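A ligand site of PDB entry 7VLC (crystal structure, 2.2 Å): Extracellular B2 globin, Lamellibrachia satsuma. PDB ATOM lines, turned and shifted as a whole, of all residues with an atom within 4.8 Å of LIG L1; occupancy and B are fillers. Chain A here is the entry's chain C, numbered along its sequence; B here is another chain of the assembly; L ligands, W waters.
NE2 of His 99 binds FE1 of LIG L1 (2.1 Å).
An oxygen (O3) of LIG L1 is in salt-bridge range of the guanidinium group (NE) of Arg 53, at 2.5 Å.
An oxygen (O1) of LIG L1 sits at hydrogen-bond distance from a ring nitrogen (NE2) of His 90 of chain B (2.9 Å).
The guanidinium group (NE) of Arg 70 lies within salt-bridge range of an oxygen (O1) of LIG L1 (3.8 Å).
O2 of LIG L1 sits at hydrogen-bond distance from NE2 of Gln 98 (3.3 Å).
An oxygen (O2) of LG2 L2 sits at hydrogen-bond distance from a ring nitrogen (NE2) of His 67, at 2.8 Å.
An iron atom (FE1) of LIG L1 is bound by an oxygen (O1) of LG2 L2, 1.8 Å away.
A ring nitrogen (ND1) of His 99 is in hydrogen-bond range of the backbone carbonyl oxygen of Leu 95 (2.7 Å).
The side-chain amide nitrogen of Gln 94 of chain B sits at hydrogen-bond distance from a ring nitrogen (NE2) of His 90 of chain B, at 3.4 Å.
The backbone carbonyl oxygen (O) of Gln 98 is in hydrogen-bond range of the guanidinium group (NE) of Arg 102.
The backbone carbonyl oxygen (O) of Phe 137 lies close to the side-chain hydroxyl (OG1) of Thr 141 (3.4 Å).
Leu 50 touches LIG L1.
Phe 51 touches LIG L1 (CE2 to C4, 3.5 Å).
CG1 of Val 54 touches O3 of LIG L1, 3.2 Å away.
His 67 touches LIG L1 (CE1 to C1, 3.8 Å).
Val 71 touches LIG L1.
Leu 75 touches LIG L1.
Arg 102 touches LIG L1 (NH2 to C32, 3.4 Å).
Gly 109 touches LIG L1 (O to C24, 3.4 Å).
CE2 of Phe 110 touches C3 of LIG L1, 3.5 Å away.
CG2 of Ile 113 touches C24 of LIG L1 (3.8 Å).
CZ of Phe 137 touches C19 of LIG L1, 3.7 Å away.
CE of Met 144 touches C14 of LIG L1 (3.5 Å).
Gln 94 of chain B touches LIG L1.
Of the 24 residues printed, 18 come within 4 Å of LIG L1.
Along chain A the residues within 4 Å of LIG L1 span positions 50 to 144.
The nearest printed residue that does not touch LIG L1 is Val 105 (4.04 Å).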
ATOM      1  N   LEU A  50      25.794 -33.974  11.994  1.00  0.00           N
ATOM      2  CA  LEU A  50      25.620 -33.063  10.863  1.00  0.00           C
ATOM      3  C   LEU A  50      26.306 -31.730  11.091  1.00  0.00           C
ATOM      4  O   LEU A  50      26.562 -31.008  10.119  1.00  0.00           O
ATOM      5  CB  LEU A  50      24.134 -32.859  10.583  1.00  0.00           C
ATOM      6  CG  LEU A  50      23.382 -34.105  10.137  1.00  0.00           C
ATOM      7  CD1 LEU A  50      21.908 -33.794  10.008  1.00  0.00           C
ATOM      8  CD2 LEU A  50      23.955 -34.614   8.821  1.00  0.00           C
ATOM      9  N   PHE A  51      26.624 -31.390  12.341  1.00  0.00           N
ATOM     10  CA  PHE A  51      27.214 -30.113  12.700  1.00  0.00           C
ATOM     11  C   PHE A  51      28.628 -30.286  13.239  1.00  0.00           C
ATOM     12  O   PHE A  51      29.068 -29.501  14.097  1.00  0.00           O
ATOM     13  CB  PHE A  51      26.333 -29.382  13.713  1.00  0.00           C
ATOM     14  CG  PHE A  51      24.881 -29.320  13.321  1.00  0.00           C
ATOM     15  CD1 PHE A  51      24.002 -30.311  13.702  1.00  0.00           C
ATOM     16  CD2 PHE A  51      24.399 -28.264  12.543  1.00  0.00           C
ATOM     17  CE1 PHE A  51      22.668 -30.261  13.328  1.00  0.00           C
ATOM     18  CE2 PHE A  51      23.077 -28.208  12.171  1.00  0.00           C
ATOM     19  CZ  PHE A  51      22.209 -29.211  12.568  1.00  0.00           C
ATOM     20  N   ARG A  53      31.272 -29.518  11.817  1.00  0.00           N
ATOM     21  CA  ARG A  53      32.077 -28.368  11.448  1.00  0.00           C
ATOM     22  C   ARG A  53      31.938 -27.223  12.452  1.00  0.00           C
ATOM     23  O   ARG A  53      32.900 -26.473  12.656  1.00  0.00           O
ATOM     24  CB  ARG A  53      31.685 -27.893  10.051  1.00  0.00           C
ATOM     25  CG  ARG A  53      32.714 -27.004   9.385  1.00  0.00           C
ATOM     26  CD  ARG A  53      32.126 -26.268   8.199  1.00  0.00           C
ATOM     27  NE  ARG A  53      31.168 -25.252   8.618  1.00  0.00           N
ATOM     28  CZ  ARG A  53      31.503 -24.016   8.946  1.00  0.00           C
ATOM     29  NH1 ARG A  53      30.564 -23.146   9.322  1.00  0.00           N
ATOM     30  NH2 ARG A  53      32.771 -23.622   8.910  1.00  0.00           N
ATOM     31  N   VAL A  54      30.777 -27.079  13.084  1.00  0.00           N
ATOM     32  CA  VAL A  54      30.536 -25.980  14.019  1.00  0.00           C
ATOM     33  C   VAL A  54      30.544 -26.473  15.464  1.00  0.00           C
ATOM     34  O   VAL A  54      29.937 -25.836  16.331  1.00  0.00           O
ATOM     35  CB  VAL A  54      29.229 -25.243  13.680  1.00  0.00           C
ATOM     36  CG1 VAL A  54      29.444 -24.307  12.492  1.00  0.00           C
ATOM     37  CG2 VAL A  54      28.104 -26.235  13.409  1.00  0.00           C
ATOM     38  N   HIS A  67      27.196 -20.390  15.029  1.00  0.00           N
ATOM     39  CA  HIS A  67      26.246 -21.097  14.186  1.00  0.00           C
ATOM     40  C   HIS A  67      24.814 -20.870  14.651  1.00  0.00           C
ATOM     41  O   HIS A  67      23.915 -20.639  13.839  1.00  0.00           O
ATOM     42  CB  HIS A  67      26.564 -22.594  14.165  1.00  0.00           C
ATOM     43  CG  HIS A  67      25.469 -23.435  13.583  1.00  0.00           C
ATOM     44  ND1 HIS A  67      25.219 -23.502  12.229  1.00  0.00           N
ATOM     45  CD2 HIS A  67      24.551 -24.230  14.180  1.00  0.00           C
ATOM     46  CE1 HIS A  67      24.202 -24.323  12.015  1.00  0.00           C
ATOM     47  NE2 HIS A  67      23.774 -24.777  13.179  1.00  0.00           N
ATOM     48  N   ARG A  70      23.574 -17.636  13.562  1.00  0.00           N
ATOM     49  CA  ARG A  70      23.252 -17.614  12.132  1.00  0.00           C
ATOM     50  C   ARG A  70      21.907 -18.265  11.862  1.00  0.00           C
ATOM     51  O   ARG A  70      21.142 -17.816  11.000  1.00  0.00           O
ATOM     52  CB  ARG A  70      24.346 -18.296  11.325  1.00  0.00           C
ATOM     53  CG  ARG A  70      25.640 -17.499  11.213  1.00  0.00           C
ATOM     54  CD  ARG A  70      26.576 -18.086  10.172  1.00  0.00           C
ATOM     55  NE  ARG A  70      26.992 -19.452  10.493  1.00  0.00           N
ATOM     56  CZ  ARG A  70      28.051 -19.749  11.238  1.00  0.00           C
ATOM     57  NH1 ARG A  70      28.802 -18.791  11.743  1.00  0.00           N
ATOM     58  NH2 ARG A  70      28.356 -21.019  11.476  1.00  0.00           N
ATOM     59  N   VAL A  71      21.587 -19.352  12.587  1.00  0.00           N
ATOM     60  CA  VAL A  71      20.314 -20.031  12.375  1.00  0.00           C
ATOM     61  C   VAL A  71      19.153 -19.140  12.793  1.00  0.00           C
ATOM     62  O   VAL A  71      18.157 -19.009  12.074  1.00  0.00           O
ATOM     63  CB  VAL A  71      20.307 -21.375  13.132  1.00  0.00           C
ATOM     64  CG1 VAL A  71      18.938 -22.027  13.031  1.00  0.00           C
ATOM     65  CG2 VAL A  71      21.375 -22.291  12.568  1.00  0.00           C
ATOM     66  N   GLY A  74      18.686 -16.342  10.404  1.00  0.00           N
ATOM     67  CA  GLY A  74      17.988 -16.788   9.209  1.00  0.00           C
ATOM     68  C   GLY A  74      16.497 -16.979   9.433  1.00  0.00           C
ATOM     69  O   GLY A  74      15.691 -16.654   8.562  1.00  0.00           O
ATOM     70  N   LEU A  75      16.128 -17.506  10.599  1.00  0.00           N
ATOM     71  CA  LEU A  75      14.714 -17.618  10.925  1.00  0.00           C
ATOM     72  C   LEU A  75      14.082 -16.246  11.126  1.00  0.00           C
ATOM     73  O   LEU A  75      12.933 -16.022  10.743  1.00  0.00           O
ATOM     74  CB  LEU A  75      14.524 -18.501  12.155  1.00  0.00           C
ATOM     75  CG  LEU A  75      13.071 -18.719  12.570  1.00  0.00           C
ATOM     76  CD1 LEU A  75      12.306 -19.475  11.478  1.00  0.00           C
ATOM     77  CD2 LEU A  75      12.965 -19.445  13.911  1.00  0.00           C
ATOM     78  N   LEU A  95      18.280 -20.374   1.312  1.00  0.00           N
ATOM     79  CA  LEU A  95      18.454 -21.252   2.461  1.00  0.00           C
ATOM     80  C   LEU A  95      18.404 -22.715   2.063  1.00  0.00           C
ATOM     81  O   LEU A  95      19.093 -23.552   2.659  1.00  0.00           O
ATOM     82  CB  LEU A  95      17.382 -20.962   3.515  1.00  0.00           C
ATOM     83  CG  LEU A  95      17.451 -19.598   4.226  1.00  0.00           C
ATOM     84  CD1 LEU A  95      16.215 -19.363   5.075  1.00  0.00           C
ATOM     85  CD2 LEU A  95      18.716 -19.506   5.069  1.00  0.00           C
ATOM     86  N   GLN A  98      21.675 -23.857   0.739  1.00  0.00           N
ATOM     87  CA  GLN A  98      22.627 -23.918   1.839  1.00  0.00           C
ATOM     88  C   GLN A  98      22.483 -25.202   2.638  1.00  0.00           C
ATOM     89  O   GLN A  98      23.466 -25.677   3.228  1.00  0.00           O
ATOM     90  CB  GLN A  98      22.465 -22.702   2.748  1.00  0.00           C
ATOM     91  CG  GLN A  98      23.092 -21.429   2.209  1.00  0.00           C
ATOM     92  CD  GLN A  98      22.920 -20.252   3.140  1.00  0.00           C
ATOM     93  OE1 GLN A  98      21.883 -20.122   3.801  1.00  0.00           O
ATOM     94  NE2 GLN A  98      23.924 -19.385   3.203  1.00  0.00           N
ATOM     95  N   HIS A  99      21.283 -25.787   2.673  1.00  0.00           N
ATOM     96  CA  HIS A  99      21.046 -27.063   3.344  1.00  0.00           C
ATOM     97  C   HIS A  99      21.101 -28.239   2.376  1.00  0.00           C
ATOM     98  O   HIS A  99      20.970 -29.387   2.801  1.00  0.00           O
ATOM     99  CB  HIS A  99      19.696 -27.035   4.071  1.00  0.00           C
ATOM    100  CG  HIS A  99      19.657 -26.077   5.218  1.00  0.00           C
ATOM    101  ND1 HIS A  99      19.551 -24.716   5.051  1.00  0.00           N
ATOM    102  CD2 HIS A  99      19.721 -26.288   6.560  1.00  0.00           C
ATOM    103  CE1 HIS A  99      19.555 -24.126   6.232  1.00  0.00           C
ATOM    104  NE2 HIS A  99      19.660 -25.061   7.160  1.00  0.00           N
ATOM    105  N   ARG A 102      24.215 -31.941   1.473  1.00  0.00           N
ATOM    106  CA  ARG A 102      24.652 -32.352   2.809  1.00  0.00           C
ATOM    107  C   ARG A 102      23.869 -33.610   3.158  1.00  0.00           C
ATOM    108  O   ARG A 102      22.693 -33.532   3.542  1.00  0.00           O
ATOM    109  CB  ARG A 102      24.422 -31.258   3.838  1.00  0.00           C
ATOM    110  CG  ARG A 102      25.207 -29.982   3.586  1.00  0.00           C
ATOM    111  CD  ARG A 102      24.878 -28.926   4.608  1.00  0.00           C
ATOM    112  NE  ARG A 102      25.435 -27.623   4.257  1.00  0.00           N
ATOM    113  CZ  ARG A 102      26.623 -27.179   4.655  1.00  0.00           C
ATOM    114  NH1 ARG A 102      27.047 -25.978   4.282  1.00  0.00           N
ATOM    115  NH2 ARG A 102      27.382 -27.931   5.437  1.00  0.00           N
ATOM    116  N   GLY A 104      22.329 -36.449   5.194  1.00  0.00           N
ATOM    117  CA  GLY A 104      21.824 -36.415   6.550  1.00  0.00           C
ATOM    118  C   GLY A 104      20.868 -35.279   6.838  1.00  0.00           C
ATOM    119  O   GLY A 104      20.133 -35.347   7.829  1.00  0.00           O
ATOM    120  N   VAL A 105      20.865 -34.243   5.994  1.00  0.00           N
ATOM    121  CA  VAL A 105      19.949 -33.121   6.141  1.00  0.00           C
ATOM    122  C   VAL A 105      18.736 -33.422   5.251  1.00  0.00           C
ATOM    123  O   VAL A 105      18.804 -33.294   4.026  1.00  0.00           O
ATOM    124  CB  VAL A 105      20.607 -31.789   5.762  1.00  0.00           C
ATOM    125  CG1 VAL A 105      19.620 -30.647   5.926  1.00  0.00           C
ATOM    126  CG2 VAL A 105      21.849 -31.563   6.605  1.00  0.00           C
ATOM    127  N   GLY A 109      14.516 -34.134   9.574  1.00  0.00           N
ATOM    128  CA  GLY A 109      15.158 -33.310  10.582  1.00  0.00           C
ATOM    129  C   GLY A 109      14.449 -31.984  10.811  1.00  0.00           C
ATOM    130  O   GLY A 109      14.459 -31.461  11.926  1.00  0.00           O
ATOM    131  N   PHE A 110      13.807 -31.450   9.766  1.00  0.00           N
ATOM    132  CA  PHE A 110      13.056 -30.208   9.929  1.00  0.00           C
ATOM    133  C   PHE A 110      11.759 -30.441  10.688  1.00  0.00           C
ATOM    134  O   PHE A 110      11.348 -29.598  11.488  1.00  0.00           O
ATOM    135  CB  PHE A 110      12.778 -29.586   8.561  1.00  0.00           C
ATOM    136  CG  PHE A 110      13.955 -28.850   7.982  1.00  0.00           C
ATOM    137  CD1 PHE A 110      14.964 -29.531   7.340  1.00  0.00           C
ATOM    138  CD2 PHE A 110      14.054 -27.470   8.103  1.00  0.00           C
ATOM    139  CE1 PHE A 110      16.052 -28.858   6.808  1.00  0.00           C
ATOM    140  CE2 PHE A 110      15.139 -26.791   7.584  1.00  0.00           C
ATOM    141  CZ  PHE A 110      16.138 -27.484   6.928  1.00  0.00           C
ATOM    142  N   ILE A 113      13.060 -30.490  14.291  1.00  0.00           N
ATOM    143  CA  ILE A 113      13.363 -29.178  14.849  1.00  0.00           C
ATOM    144  C   ILE A 113      12.086 -28.353  14.970  1.00  0.00           C
ATOM    145  O   ILE A 113      11.995 -27.469  15.828  1.00  0.00           O
ATOM    146  CB  ILE A 113      14.430 -28.455  14.001  1.00  0.00           C
ATOM    147  CG1 ILE A 113      15.147 -27.398  14.846  1.00  0.00           C
ATOM    148  CG2 ILE A 113      13.819 -27.815  12.761  1.00  0.00           C
ATOM    149  CD1 ILE A 113      16.289 -26.719  14.136  1.00  0.00           C
ATOM    150  N   PHE A 117      11.142 -26.373  18.382  1.00  0.00           N
ATOM    151  CA  PHE A 117      10.628 -25.023  18.580  1.00  0.00           C
ATOM    152  C   PHE A 117       9.289 -25.030  19.325  1.00  0.00           C
ATOM    153  O   PHE A 117       9.029 -24.156  20.159  1.00  0.00           O
ATOM    154  CB  PHE A 117      10.490 -24.303  17.246  1.00  0.00           C
ATOM    155  CG  PHE A 117      11.741 -23.632  16.765  1.00  0.00           C
ATOM    156  CD1 PHE A 117      12.078 -22.368  17.211  1.00  0.00           C
ATOM    157  CD2 PHE A 117      12.576 -24.270  15.867  1.00  0.00           C
ATOM    158  CE1 PHE A 117      13.238 -21.751  16.773  1.00  0.00           C
ATOM    159  CE2 PHE A 117      13.739 -23.659  15.417  1.00  0.00           C
ATOM    160  CZ  PHE A 117      14.071 -22.403  15.872  1.00  0.00           C
ATOM    161  N   PHE A 137       5.562 -21.613  10.519  1.00  0.00           N
ATOM    162  CA  PHE A 137       6.849 -22.279  10.581  1.00  0.00           C
ATOM    163  C   PHE A 137       6.958 -23.363   9.510  1.00  0.00           C
ATOM    164  O   PHE A 137       7.999 -23.487   8.856  1.00  0.00           O
ATOM    165  CB  PHE A 137       7.071 -22.883  11.972  1.00  0.00           C
ATOM    166  CG  PHE A 137       8.452 -23.420  12.201  1.00  0.00           C
ATOM    167  CD1 PHE A 137       8.769 -24.738  11.895  1.00  0.00           C
ATOM    168  CD2 PHE A 137       9.447 -22.597  12.720  1.00  0.00           C
ATOM    169  CE1 PHE A 137      10.042 -25.227  12.101  1.00  0.00           C
ATOM    170  CE2 PHE A 137      10.740 -23.084  12.940  1.00  0.00           C
ATOM    171  CZ  PHE A 137      11.029 -24.404  12.625  1.00  0.00           C
ATOM    172  N   THR A 141       9.593 -23.751   6.419  1.00  0.00           N
ATOM    173  CA  THR A 141      10.401 -24.942   6.140  1.00  0.00           C
ATOM    174  C   THR A 141      10.043 -25.596   4.811  1.00  0.00           C
ATOM    175  O   THR A 141      10.902 -26.270   4.231  1.00  0.00           O
ATOM    176  CB  THR A 141      10.271 -25.960   7.278  1.00  0.00           C
ATOM    177  OG1 THR A 141       8.907 -26.392   7.389  1.00  0.00           O
ATOM    178  CG2 THR A 141      10.728 -25.361   8.597  1.00  0.00           C
ATOM    179  N   MET A 144      12.424 -24.272   2.533  1.00  0.00           N
ATOM    180  CA  MET A 144      13.798 -24.649   2.843  1.00  0.00           C
ATOM    181  C   MET A 144      14.107 -26.102   2.488  1.00  0.00           C
ATOM    182  O   MET A 144      15.285 -26.465   2.411  1.00  0.00           O
ATOM    183  CB  MET A 144      14.085 -24.430   4.327  1.00  0.00           C
ATOM    184  CG  MET A 144      13.934 -22.992   4.802  1.00  0.00           C
ATOM    185  SD  MET A 144      14.424 -22.812   6.533  1.00  0.00           S
ATOM    186  CE  MET A 144      16.174 -23.193   6.427  1.00  0.00           C
ATOM    187  N   HIS B  90      33.521 -16.017   9.520  1.00  0.00           N
ATOM    188  CA  HIS B  90      32.561 -16.662   8.624  1.00  0.00           C
ATOM    189  C   HIS B  90      32.179 -15.743   7.480  1.00  0.00           C
ATOM    190  O   HIS B  90      32.052 -16.193   6.329  1.00  0.00           O
ATOM    191  CB  HIS B  90      31.320 -17.083   9.416  1.00  0.00           C
ATOM    192  CG  HIS B  90      30.381 -17.959   8.649  1.00  0.00           C
ATOM    193  ND1 HIS B  90      30.476 -19.329   8.648  1.00  0.00           N
ATOM    194  CD2 HIS B  90      29.326 -17.652   7.853  1.00  0.00           C
ATOM    195  CE1 HIS B  90      29.518 -19.833   7.884  1.00  0.00           C
ATOM    196  NE2 HIS B  90      28.805 -18.839   7.397  1.00  0.00           N
ATOM    197  N   GLN B  94      32.879 -15.974   3.229  1.00  0.00           N
ATOM    198  CA  GLN B  94      31.801 -15.762   2.266  1.00  0.00           C
ATOM    199  C   GLN B  94      32.168 -14.732   1.205  1.00  0.00           C
ATOM    200  O   GLN B  94      31.501 -14.676   0.165  1.00  0.00           O
ATOM    201  CB  GLN B  94      30.527 -15.332   2.997  1.00  0.00           C
ATOM    202  CG  GLN B  94      29.922 -16.432   3.870  1.00  0.00           C
ATOM    203  CD  GLN B  94      28.774 -15.944   4.743  1.00  0.00           C
ATOM    204  OE1 GLN B  94      28.782 -14.813   5.231  1.00  0.00           O
ATOM    205  NE2 GLN B  94      27.773 -16.798   4.947  1.00  0.00           N
HETATM  206  C1  LIG L   1      23.550 -24.023   8.331  1.00  0.00           C
HETATM  207  C2  LIG L   1      19.225 -21.883   8.963  1.00  0.00           C
HETATM  208  C3  LIG L   1      17.276 -26.151  10.218  1.00  0.00           C
HETATM  209  C4  LIG L   1      21.451 -28.351   9.029  1.00  0.00           C
HETATM  210  C5  LIG L   1      22.561 -23.062   8.420  1.00  0.00           C
HETATM  211  C6  LIG L   1      22.730 -21.629   8.221  1.00  0.00           C
HETATM  212  C7  LIG L   1      21.541 -21.056   8.389  1.00  0.00           C
HETATM  213  C8  LIG L   1      20.569 -22.083   8.716  1.00  0.00           C
HETATM  214  C9  LIG L   1      21.240 -19.534   8.269  1.00  0.00           C
HETATM  215  C10 LIG L   1      24.044 -20.887   7.858  1.00  0.00           C
HETATM  216  C11 LIG L   1      24.540 -21.292   6.474  1.00  0.00           C
HETATM  217  C12 LIG L   1      25.717 -20.447   6.080  1.00  0.00           C
HETATM  218  O1  LIG L   1      26.061 -19.495   6.821  1.00  0.00           O
HETATM  219  O2  LIG L   1      26.330 -20.718   5.011  1.00  0.00           O
HETATM  220  C13 LIG L   1      18.332 -22.839   9.397  1.00  0.00           C
HETATM  221  C14 LIG L   1      16.951 -22.598   9.791  1.00  0.00           C
HETATM  222  C15 LIG L   1      16.409 -23.787  10.145  1.00  0.00           C
HETATM  223  C16 LIG L   1      17.431 -24.803   9.978  1.00  0.00           C
HETATM  224  C17 LIG L   1      16.304 -21.193   9.796  1.00  0.00           C
HETATM  225  C18 LIG L   1      14.985 -24.128  10.646  1.00  0.00           C
HETATM  226  C19 LIG L   1      13.972 -23.254  10.717  1.00  0.00           C
HETATM  227  C20 LIG L   1      18.234 -27.128  10.006  1.00  0.00           C
HETATM  228  C21 LIG L   1      18.090 -28.546  10.263  1.00  0.00           C
HETATM  229  C22 LIG L   1      19.240 -29.155   9.938  1.00  0.00           C
HETATM  230  C23 LIG L   1      20.151 -28.135   9.459  1.00  0.00           C
HETATM  231  C24 LIG L   1      16.784 -29.168  10.825  1.00  0.00           C
HETATM  232  C25 LIG L   1      19.631 -30.659  10.014  1.00  0.00           C
HETATM  233  C26 LIG L   1      18.829 -31.647  10.442  1.00  0.00           C
HETATM  234  C27 LIG L   1      22.391 -27.384   8.765  1.00  0.00           C
HETATM  235  C28 LIG L   1      23.796 -27.603   8.465  1.00  0.00           C
HETATM  236  C29 LIG L   1      24.373 -26.407   8.279  1.00  0.00           C
HETATM  237  C30 LIG L   1      23.357 -25.387   8.453  1.00  0.00           C
HETATM  238  C31 LIG L   1      24.497 -28.977   8.375  1.00  0.00           C
HETATM  239  C32 LIG L   1      25.844 -26.138   7.927  1.00  0.00           C
HETATM  240  C33 LIG L   1      26.712 -26.232   9.174  1.00  0.00           C
HETATM  241  C34 LIG L   1      27.980 -25.449   8.963  1.00  0.00           C
HETATM  242  O3  LIG L   1      28.988 -25.735   9.648  1.00  0.00           O
HETATM  243  O4  LIG L   1      27.973 -24.531   8.097  1.00  0.00           O
HETATM  244  N1  LIG L   1      21.238 -23.297   8.723  1.00  0.00           N
HETATM  245  N2  LIG L   1      18.578 -24.188   9.522  1.00  0.00           N
HETATM  246  N3  LIG L   1      19.506 -26.906   9.508  1.00  0.00           N
HETATM  247  N4  LIG L   1      22.164 -26.021   8.744  1.00  0.00           N
HETATM  248 FE1  LIG L   1      20.334 -25.092   9.112  1.00  0.00          FE
HETATM  249  O1  LG2 L   2      20.750 -25.116  10.860  1.00  0.00           O
HETATM  250  O2  LG2 L   2      21.541 -25.569  11.652  1.00  0.00           O
HETATM  251  O   HOH W   1      24.085 -17.287   7.541  1.00  0.00           O
HETATM  252  O   HOH W   2      20.182 -16.660   6.855  1.00  0.00           O
HETATM  253  O   HOH W   3      21.921 -16.299   8.915  1.00  0.00           O
